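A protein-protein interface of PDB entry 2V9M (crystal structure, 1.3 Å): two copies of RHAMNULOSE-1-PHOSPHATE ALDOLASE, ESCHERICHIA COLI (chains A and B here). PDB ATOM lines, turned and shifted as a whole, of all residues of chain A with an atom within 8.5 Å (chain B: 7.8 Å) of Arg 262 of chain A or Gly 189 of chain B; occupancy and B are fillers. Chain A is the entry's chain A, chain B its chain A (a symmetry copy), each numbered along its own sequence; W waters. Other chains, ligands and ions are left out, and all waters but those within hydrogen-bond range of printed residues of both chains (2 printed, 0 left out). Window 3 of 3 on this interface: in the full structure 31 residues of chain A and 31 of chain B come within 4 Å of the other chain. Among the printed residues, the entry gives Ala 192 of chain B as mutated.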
ATOM      1  N   THR A 170     -23.545  18.882 -21.752  1.00  0.00           N
ATOM      2  CA  THR A 170     -22.664  20.061 -21.619  1.00  0.00           C
ATOM      3  C   THR A 170     -23.366  21.305 -21.110  1.00  0.00           C
ATOM      4  O   THR A 170     -22.810  22.059 -20.318  1.00  0.00           O
ATOM      5  CB  THR A 170     -21.969  20.320 -22.970  1.00  0.00           C
ATOM      6  OG1 THR A 170     -20.957  19.337 -23.186  1.00  0.00           O
ATOM      7  CG2 THR A 170     -21.292  21.675 -23.006  1.00  0.00           C
ATOM      8  N   LEU A 173     -24.355  22.838 -16.695  1.00  0.00           N
ATOM      9  CA  LEU A 173     -23.709  23.821 -15.804  1.00  0.00           C
ATOM     10  C   LEU A 173     -24.196  25.239 -16.106  1.00  0.00           C
ATOM     11  O   LEU A 173     -24.311  26.059 -15.208  1.00  0.00           O
ATOM     12  CB  LEU A 173     -22.179  23.648 -15.891  1.00  0.00           C
ATOM     13  CG  LEU A 173     -21.306  24.614 -15.094  1.00  0.00           C
ATOM     14  CD1 LEU A 173     -19.984  23.976 -14.656  1.00  0.00           C
ATOM     15  CD2 LEU A 173     -20.961  25.834 -15.920  1.00  0.00           C
ATOM     16  N   VAL A 174     -24.441  25.531 -17.375  1.00  0.00           N
ATOM     17  CA  VAL A 174     -24.884  26.863 -17.734  1.00  0.00           C
ATOM     18  C   VAL A 174     -26.354  27.086 -17.364  1.00  0.00           C
ATOM     19  O   VAL A 174     -26.743  28.199 -16.967  1.00  0.00           O
ATOM     20  CB  VAL A 174     -24.625  27.092 -19.242  1.00  0.00           C
ATOM     21  CG1 VAL A 174     -25.137  28.465 -19.695  1.00  0.00           C
ATOM     22  CG2 VAL A 174     -23.134  26.919 -19.583  1.00  0.00           C
ATOM     23  N   GLU A 255     -12.629  21.526 -17.791  1.00  0.00           N
ATOM     24  CA  GLU A 255     -13.566  21.872 -18.860  1.00  0.00           C
ATOM     25  C   GLU A 255     -14.770  22.573 -18.281  1.00  0.00           C
ATOM     26  O   GLU A 255     -15.244  23.566 -18.845  1.00  0.00           O
ATOM     27  CB  GLU A 255     -13.913  20.611 -19.690  1.00  0.00           C
ATOM     28  CG  GLU A 255     -12.750  20.130 -20.537  1.00  0.00           C
ATOM     29  CD  GLU A 255     -12.828  18.730 -21.119  1.00  0.00           C
ATOM     30  OE1 GLU A 255     -12.090  18.430 -22.118  1.00  0.00           O
ATOM     31  OE2 GLU A 255     -13.593  17.905 -20.578  1.00  0.00           O
ATOM     32  N   LEU A 256     -15.286  22.059 -17.143  1.00  0.00           N
ATOM     33  CA  LEU A 256     -16.436  22.686 -16.480  1.00  0.00           C
ATOM     34  C   LEU A 256     -16.067  24.099 -16.025  1.00  0.00           C
ATOM     35  O   LEU A 256     -16.854  25.035 -16.199  1.00  0.00           O
ATOM     36  CB  LEU A 256     -16.930  21.867 -15.308  1.00  0.00           C
ATOM     37  CG  LEU A 256     -17.554  20.502 -15.663  1.00  0.00           C
ATOM     38  CD1 LEU A 256     -17.704  19.675 -14.400  1.00  0.00           C
ATOM     39  CD2 LEU A 256     -18.906  20.652 -16.336  1.00  0.00           C
ATOM     40  N   ILE A 257     -14.848  24.283 -15.507  1.00  0.00           N
ATOM     41  CA  ILE A 257     -14.396  25.647 -15.153  1.00  0.00           C
ATOM     42  C   ILE A 257     -14.366  26.592 -16.343  1.00  0.00           C
ATOM     43  O   ILE A 257     -14.879  27.699 -16.260  1.00  0.00           O
ATOM     44  CB  ILE A 257     -13.026  25.563 -14.476  1.00  0.00           C
ATOM     45  CG1 ILE A 257     -13.171  24.893 -13.100  1.00  0.00           C
ATOM     46  CG2 ILE A 257     -12.371  26.931 -14.339  1.00  0.00           C
ATOM     47  CD1 ILE A 257     -11.874  24.529 -12.419  1.00  0.00           C
ATOM     48  N   ALA A 258     -13.819  26.162 -17.476  1.00  0.00           N
ATOM     49  CA  ALA A 258     -13.763  26.941 -18.702  1.00  0.00           C
ATOM     50  C   ALA A 258     -15.139  27.293 -19.265  1.00  0.00           C
ATOM     51  O   ALA A 258     -15.399  28.407 -19.731  1.00  0.00           O
ATOM     52  CB  ALA A 258     -12.988  26.209 -19.800  1.00  0.00           C
ATOM     53  N   LEU A 259     -16.047  26.303 -19.205  1.00  0.00           N
ATOM     54  CA  LEU A 259     -17.448  26.486 -19.585  1.00  0.00           C
ATOM     55  C   LEU A 259     -18.104  27.584 -18.735  1.00  0.00           C
ATOM     56  O   LEU A 259     -18.743  28.488 -19.261  1.00  0.00           O
ATOM     57  CB  LEU A 259     -18.175  25.155 -19.400  1.00  0.00           C
ATOM     58  CG  LEU A 259     -19.633  25.088 -19.827  1.00  0.00           C
ATOM     59  CD1 LEU A 259     -19.838  25.343 -21.292  1.00  0.00           C
ATOM     60  CD2 LEU A 259     -20.210  23.725 -19.430  1.00  0.00           C
ATOM     61  N   GLY A 260     -17.930  27.529 -17.413  1.00  0.00           N
ATOM     62  CA  GLY A 260     -18.560  28.532 -16.574  1.00  0.00           C
ATOM     63  C   GLY A 260     -17.983  29.915 -16.835  1.00  0.00           C
ATOM     64  O   GLY A 260     -18.701  30.912 -16.831  1.00  0.00           O
ATOM     65  N   LYS A 261     -16.669  29.997 -17.058  1.00  0.00           N
ATOM     66  CA  LYS A 261     -16.126  31.333 -17.333  1.00  0.00           C
ATOM     67  C   LYS A 261     -16.661  31.881 -18.646  1.00  0.00           C
ATOM     68  O   LYS A 261     -17.003  33.060 -18.773  1.00  0.00           O
ATOM     69  CB  LYS A 261     -14.607  31.249 -17.399  1.00  0.00           C
ATOM     70  CG  LYS A 261     -13.936  30.876 -16.090  1.00  0.00           C
ATOM     71  CD  LYS A 261     -12.423  31.009 -16.246  1.00  0.00           C
ATOM     72  CE  LYS A 261     -11.639  30.370 -15.110  1.00  0.00           C
ATOM     73  NZ  LYS A 261     -12.278  30.661 -13.788  1.00  0.00           N
ATOM     74  N   ARG A 262     -16.746  31.048 -19.682  1.00  0.00           N
ATOM     75  CA  ARG A 262     -17.182  31.553 -20.973  1.00  0.00           C
ATOM     76  C   ARG A 262     -18.603  32.099 -20.893  1.00  0.00           C
ATOM     77  O   ARG A 262     -18.934  33.107 -21.512  1.00  0.00           O
ATOM     78  CB  ARG A 262     -17.134  30.422 -21.988  1.00  0.00           C
ATOM     79  CG  ARG A 262     -17.708  30.763 -23.346  1.00  0.00           C
ATOM     80  CD  ARG A 262     -16.919  31.783 -24.152  1.00  0.00           C
ATOM     81  NE  ARG A 262     -17.549  32.027 -25.433  1.00  0.00           N
ATOM     82  CZ  ARG A 262     -16.984  32.762 -26.403  1.00  0.00           C
ATOM     83  NH1 ARG A 262     -15.788  33.304 -26.189  1.00  0.00           N
ATOM     84  NH2 ARG A 262     -17.595  32.957 -27.567  1.00  0.00           N
ATOM     85  N   PHE A 263     -19.454  31.402 -20.122  1.00  0.00           N
ATOM     86  CA  PHE A 263     -20.873  31.736 -20.042  1.00  0.00           C
ATOM     87  C   PHE A 263     -21.195  32.658 -18.875  1.00  0.00           C
ATOM     88  O   PHE A 263     -22.367  33.006 -18.686  1.00  0.00           O
ATOM     89  CB  PHE A 263     -21.765  30.451 -19.983  1.00  0.00           C
ATOM     90  CG  PHE A 263     -21.841  29.869 -21.391  1.00  0.00           C
ATOM     91  CD1 PHE A 263     -20.930  28.966 -21.885  1.00  0.00           C
ATOM     92  CD2 PHE A 263     -22.865  30.260 -22.248  1.00  0.00           C
ATOM     93  CE1 PHE A 263     -20.947  28.469 -23.196  1.00  0.00           C
ATOM     94  CE2 PHE A 263     -22.897  29.787 -23.545  1.00  0.00           C
ATOM     95  CZ  PHE A 263     -21.976  28.883 -24.028  1.00  0.00           C
ATOM     96  N   GLY A 264     -20.160  33.074 -18.121  1.00  0.00           N
ATOM     97  CA  GLY A 264     -20.324  34.062 -17.083  1.00  0.00           C
ATOM     98  C   GLY A 264     -21.201  33.585 -15.952  1.00  0.00           C
ATOM     99  O   GLY A 264     -21.988  34.324 -15.393  1.00  0.00           O
ATOM    100  N   VAL A 265     -21.095  32.328 -15.562  1.00  0.00           N
ATOM    101  CA  VAL A 265     -21.805  31.820 -14.382  1.00  0.00           C
ATOM    102  C   VAL A 265     -20.787  31.349 -13.350  1.00  0.00           C
ATOM    103  O   VAL A 265     -19.670  31.000 -13.702  1.00  0.00           O
ATOM    104  CB  VAL A 265     -22.757  30.676 -14.733  1.00  0.00           C
ATOM    105  CG1 VAL A 265     -23.830  31.199 -15.659  1.00  0.00           C
ATOM    106  CG2 VAL A 265     -21.987  29.503 -15.350  1.00  0.00           C
ATOM    107  N   SER B 116     -27.107  34.692 -33.195  1.00  0.00           N
ATOM    108  CA  SER B 116     -25.782  34.506 -32.685  1.00  0.00           C
ATOM    109  C   SER B 116     -25.012  33.278 -33.201  1.00  0.00           C
ATOM    110  O   SER B 116     -23.786  33.371 -33.320  1.00  0.00           O
ATOM    111  CB  SER B 116     -25.781  34.312 -31.158  1.00  0.00           C
ATOM    112  OG  SER B 116     -26.476  35.298 -30.417  1.00  0.00           O
ATOM    113  N   GLU B 117     -25.636  32.143 -33.443  1.00  0.00           N
ATOM    114  CA  GLU B 117     -24.975  30.917 -33.893  1.00  0.00           C
ATOM    115  C   GLU B 117     -24.814  30.891 -35.403  1.00  0.00           C
ATOM    116  O   GLU B 117     -24.216  29.979 -35.997  1.00  0.00           O
ATOM    117  CB  GLU B 117     -25.754  29.687 -33.422  1.00  0.00           C
ATOM    118  CG  GLU B 117     -25.561  29.308 -31.960  1.00  0.00           C
ATOM    119  CD  GLU B 117     -26.661  29.735 -31.009  1.00  0.00           C
ATOM    120  OE1 GLU B 117     -26.751  30.988 -30.868  1.00  0.00           O
ATOM    121  OE2 GLU B 117     -27.441  28.962 -30.368  1.00  0.00           O
ATOM    122  N   ALA B 120     -21.135  30.531 -36.909  1.00  0.00           N
ATOM    123  CA  ALA B 120     -20.634  29.139 -36.951  1.00  0.00           C
ATOM    124  C   ALA B 120     -21.335  28.284 -37.997  1.00  0.00           C
ATOM    125  O   ALA B 120     -20.734  27.466 -38.686  1.00  0.00           O
ATOM    126  CB  ALA B 120     -20.789  28.450 -35.611  1.00  0.00           C
ATOM    127  N   MET B 186     -15.145  20.643 -26.552  1.00  0.00           N
ATOM    128  CA  MET B 186     -14.783  22.054 -26.673  1.00  0.00           C
ATOM    129  C   MET B 186     -15.886  22.894 -26.060  1.00  0.00           C
ATOM    130  O   MET B 186     -17.062  22.544 -26.104  1.00  0.00           O
ATOM    131  CB  MET B 186     -14.543  22.487 -28.130  1.00  0.00           C
ATOM    132  CG  MET B 186     -13.439  21.689 -28.793  1.00  0.00           C
ATOM    133  SD  MET B 186     -13.166  22.089 -30.517  1.00  0.00           S
ATOM    134  CE  MET B 186     -12.432  23.720 -30.418  1.00  0.00           C
ATOM    135  N   VAL B 187     -15.498  24.055 -25.558  1.00  0.00           N
ATOM    136  CA  VAL B 187     -16.494  25.028 -25.068  1.00  0.00           C
ATOM    137  C   VAL B 187     -17.413  25.463 -26.230  1.00  0.00           C
ATOM    138  O   VAL B 187     -16.929  25.895 -27.287  1.00  0.00           O
ATOM    139  CB  VAL B 187     -15.786  26.234 -24.447  1.00  0.00           C
ATOM    140  CG1 VAL B 187     -16.856  27.257 -24.064  1.00  0.00           C
ATOM    141  CG2 VAL B 187     -14.939  25.817 -23.241  1.00  0.00           C
ATOM    142  N   PRO B 188     -18.748  25.332 -26.112  1.00  0.00           N
ATOM    143  CA  PRO B 188     -19.618  25.709 -27.209  1.00  0.00           C
ATOM    144  C   PRO B 188     -19.701  27.221 -27.402  1.00  0.00           C
ATOM    145  O   PRO B 188     -19.439  28.034 -26.518  1.00  0.00           O
ATOM    146  CB  PRO B 188     -20.980  25.175 -26.843  1.00  0.00           C
ATOM    147  CG  PRO B 188     -20.864  24.528 -25.538  1.00  0.00           C
ATOM    148  CD  PRO B 188     -19.499  24.780 -24.982  1.00  0.00           C
ATOM    149  N   GLY B 189     -20.101  27.560 -28.633  1.00  0.00           N
ATOM    150  CA  GLY B 189     -20.342  28.951 -28.974  1.00  0.00           C
ATOM    151  C   GLY B 189     -19.075  29.737 -29.349  1.00  0.00           C
ATOM    152  O   GLY B 189     -19.179  30.935 -29.622  1.00  0.00           O
ATOM    153  N   THR B 190     -17.902  29.135 -29.365  1.00  0.00           N
ATOM    154  CA  THR B 190     -16.630  29.790 -29.557  1.00  0.00           C
ATOM    155  C   THR B 190     -16.210  29.701 -31.015  1.00  0.00           C
ATOM    156  O   THR B 190     -16.657  28.863 -31.772  1.00  0.00           O
ATOM    157  CB  THR B 190     -15.490  29.156 -28.724  1.00  0.00           C
ATOM    158  OG1 THR B 190     -15.340  27.796 -29.187  1.00  0.00           O
ATOM    159  CG2 THR B 190     -15.837  29.177 -27.255  1.00  0.00           C
ATOM    160  N   ASP B 191     -15.304  30.608 -31.361  1.00  0.00           N
ATOM    161  CA  ASP B 191     -14.784  30.599 -32.726  1.00  0.00           C
ATOM    162  C   ASP B 191     -14.097  29.256 -32.938  1.00  0.00           C
ATOM    163  O   ASP B 191     -14.179  28.654 -34.016  1.00  0.00           O
ATOM    164  CB  ASP B 191     -13.909  31.840 -32.919  1.00  0.00           C
ATOM    165  CG  ASP B 191     -14.695  33.109 -33.173  1.00  0.00           C
ATOM    166  OD1 ASP B 191     -15.946  33.076 -33.227  1.00  0.00           O
ATOM    167  OD2 ASP B 191     -14.100  34.196 -33.361  1.00  0.00           O
ATOM    168  N   ALA B 192     -13.432  28.759 -31.896  1.00  0.00           N
ATOM    169  CA  ALA B 192     -12.668  27.516 -31.974  1.00  0.00           C
ATOM    170  C   ALA B 192     -13.555  26.339 -32.362  1.00  0.00           C
ATOM    171  O   ALA B 192     -13.188  25.583 -33.272  1.00  0.00           O
ATOM    172  CB  ALA B 192     -11.965  27.252 -30.647  1.00  0.00           C
ATOM    173  N   ILE B 193     -14.699  26.192 -31.680  1.00  0.00           N
ATOM    174  CA  ILE B 193     -15.511  25.039 -32.009  1.00  0.00           C
ATOM    175  C   ILE B 193     -16.173  25.196 -33.373  1.00  0.00           C
ATOM    176  O   ILE B 193     -16.376  24.206 -34.091  1.00  0.00           O
ATOM    177  CB  ILE B 193     -16.549  24.735 -30.912  1.00  0.00           C
ATOM    178  CG1 ILE B 193     -17.110  23.328 -31.055  1.00  0.00           C
ATOM    179  CG2 ILE B 193     -17.635  25.776 -30.874  1.00  0.00           C
ATOM    180  CD1 ILE B 193     -18.026  22.948 -29.878  1.00  0.00           C
ATOM    181  N   GLY B 194     -16.505  26.415 -33.766  1.00  0.00           N
ATOM    182  CA  GLY B 194     -17.081  26.642 -35.101  1.00  0.00           C
ATOM    183  C   GLY B 194     -16.100  26.312 -36.215  1.00  0.00           C
ATOM    184  O   GLY B 194     -16.458  25.651 -37.206  1.00  0.00           O
ATOM    185  N   TRP B 209     -19.948  16.152 -31.155  1.00  0.00           N
ATOM    186  CA  TRP B 209     -19.423  16.919 -30.046  1.00  0.00           C
ATOM    187  C   TRP B 209     -19.594  16.082 -28.774  1.00  0.00           C
ATOM    188  O   TRP B 209     -20.719  15.941 -28.291  1.00  0.00           O
ATOM    189  CB  TRP B 209     -20.205  18.226 -29.940  1.00  0.00           C
ATOM    190  CG  TRP B 209     -19.952  19.228 -31.033  1.00  0.00           C
ATOM    191  CD1 TRP B 209     -19.089  19.162 -32.089  1.00  0.00           C
ATOM    192  CD2 TRP B 209     -20.611  20.491 -31.127  1.00  0.00           C
ATOM    193  NE1 TRP B 209     -19.172  20.303 -32.842  1.00  0.00           N
ATOM    194  CE2 TRP B 209     -20.097  21.140 -32.258  1.00  0.00           C
ATOM    195  CE3 TRP B 209     -21.569  21.154 -30.350  1.00  0.00           C
ATOM    196  CZ2 TRP B 209     -20.488  22.385 -32.670  1.00  0.00           C
ATOM    197  CZ3 TRP B 209     -21.978  22.412 -30.742  1.00  0.00           C
ATOM    198  CH2 TRP B 209     -21.438  23.034 -31.877  1.00  0.00           C
ATOM    199  N   HIS B 212     -22.261  16.256 -25.687  1.00  0.00           N
ATOM    200  CA  HIS B 212     -23.066  17.404 -26.132  1.00  0.00           C
ATOM    201  C   HIS B 212     -24.007  16.955 -27.239  1.00  0.00           C
ATOM    202  O   HIS B 212     -25.224  17.097 -27.031  1.00  0.00           O
ATOM    203  CB  HIS B 212     -22.144  18.568 -26.537  1.00  0.00           C
ATOM    204  CG  HIS B 212     -22.865  19.821 -26.935  1.00  0.00           C
ATOM    205  ND1 HIS B 212     -22.276  21.049 -26.975  1.00  0.00           N
ATOM    206  CD2 HIS B 212     -24.147  20.117 -27.328  1.00  0.00           C
ATOM    207  CE1 HIS B 212     -23.149  21.958 -27.363  1.00  0.00           C
ATOM    208  NE2 HIS B 212     -24.328  21.424 -27.599  1.00  0.00           N
HETATM  209  O   HOH W   1     -19.891  30.643 -26.213  1.00  0.00           O
HETATM  210  O   HOH W   2     -14.545  32.643 -29.388  1.00  0.00           O
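NH2 of Arg 262 of chain A sits at hydrogen-bond distance from O of Gly 189 of chain B (3.3 Å).
OG1 of Thr 190 of chain B is in hydrogen-bond range of N of Ile 193 of chain B.
The backbone carbonyl oxygen (O) of Val 187 of chain B sits at hydrogen-bond distance from the side-chain hydroxyl (OG1) of Thr 190 of chain B (3.1 Å).
The side-chain hydroxyl (OG1) of Thr 190 of chain B lies close to the backbone NH (N) of Ala 192 of chain B (3.5 Å).
Among the printed residues, merely in contact across the chains: Thr 170 of chain A with His 212 of chain B (3.6 Å), Phe 263 of chain A with Pro 188 of chain B (3.7 Å), Arg 262 of chain A with Val 187 of chain B (3.7 Å), Leu 259 of chain A with Pro 188 of chain B (3.7 Å), Arg 262 of chain A with Thr 190 of chain B (3.8 Å), Thr 170 of chain A with Pro 188 of chain B (3.8 Å) and Ala 258 of chain A with Val 187 of chain B (3.97 Å).
Arg 262 of chain A touches just these residues of chain B: Val 187 (3.7 Å), Gly 189 (3.3 Å) and Thr 190 (3.8 Å).
Of the printed residues of chain B, Phe 263 of chain A touches Pro 188 (3.7 Å).
Printed residues of chain A within 4 Å of Pro 188 of chain B: Thr 170, Leu 259 and Phe 263.
Gly 189 of chain B touches one residue of chain A.
Of chain A, only Arg 262 comes within 4 Å of Thr 190 of chain B.
Ile 193 of chain B touches none of the printed residues of chain A.
The nearest residue of chain B that does not touch Arg 262 of chain A is Pro 188 of chain B (4.5 Å).
The nearest residue of chain A that does not touch Gly 189 of chain B is Phe 263 of chain A (5.1 Å).
Of the 14 printed residues of chain B, 5 touch a printed residue of chain A.
Printed residues of chain B that touch a printed residue of chain A: Val 187, Pro 188, Gly 189, Thr 190 and His 212.
Among the printed residues, no Asp or Glu carboxylate lies within 4 Å of a Lys or Arg side-chain nitrogen of the other chain.
No position is printed for both chains.
Water W1 lies within hydrogen-bond range of O of Pro 188 of chain B, NE of Arg 262 of chain A and O of Gly 189 of chain B.
Water W2 lies within hydrogen-bond range of N of Asp 191 of chain B (2.9 Å) and NH1 of Arg 262 of chain A (3.5 Å).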
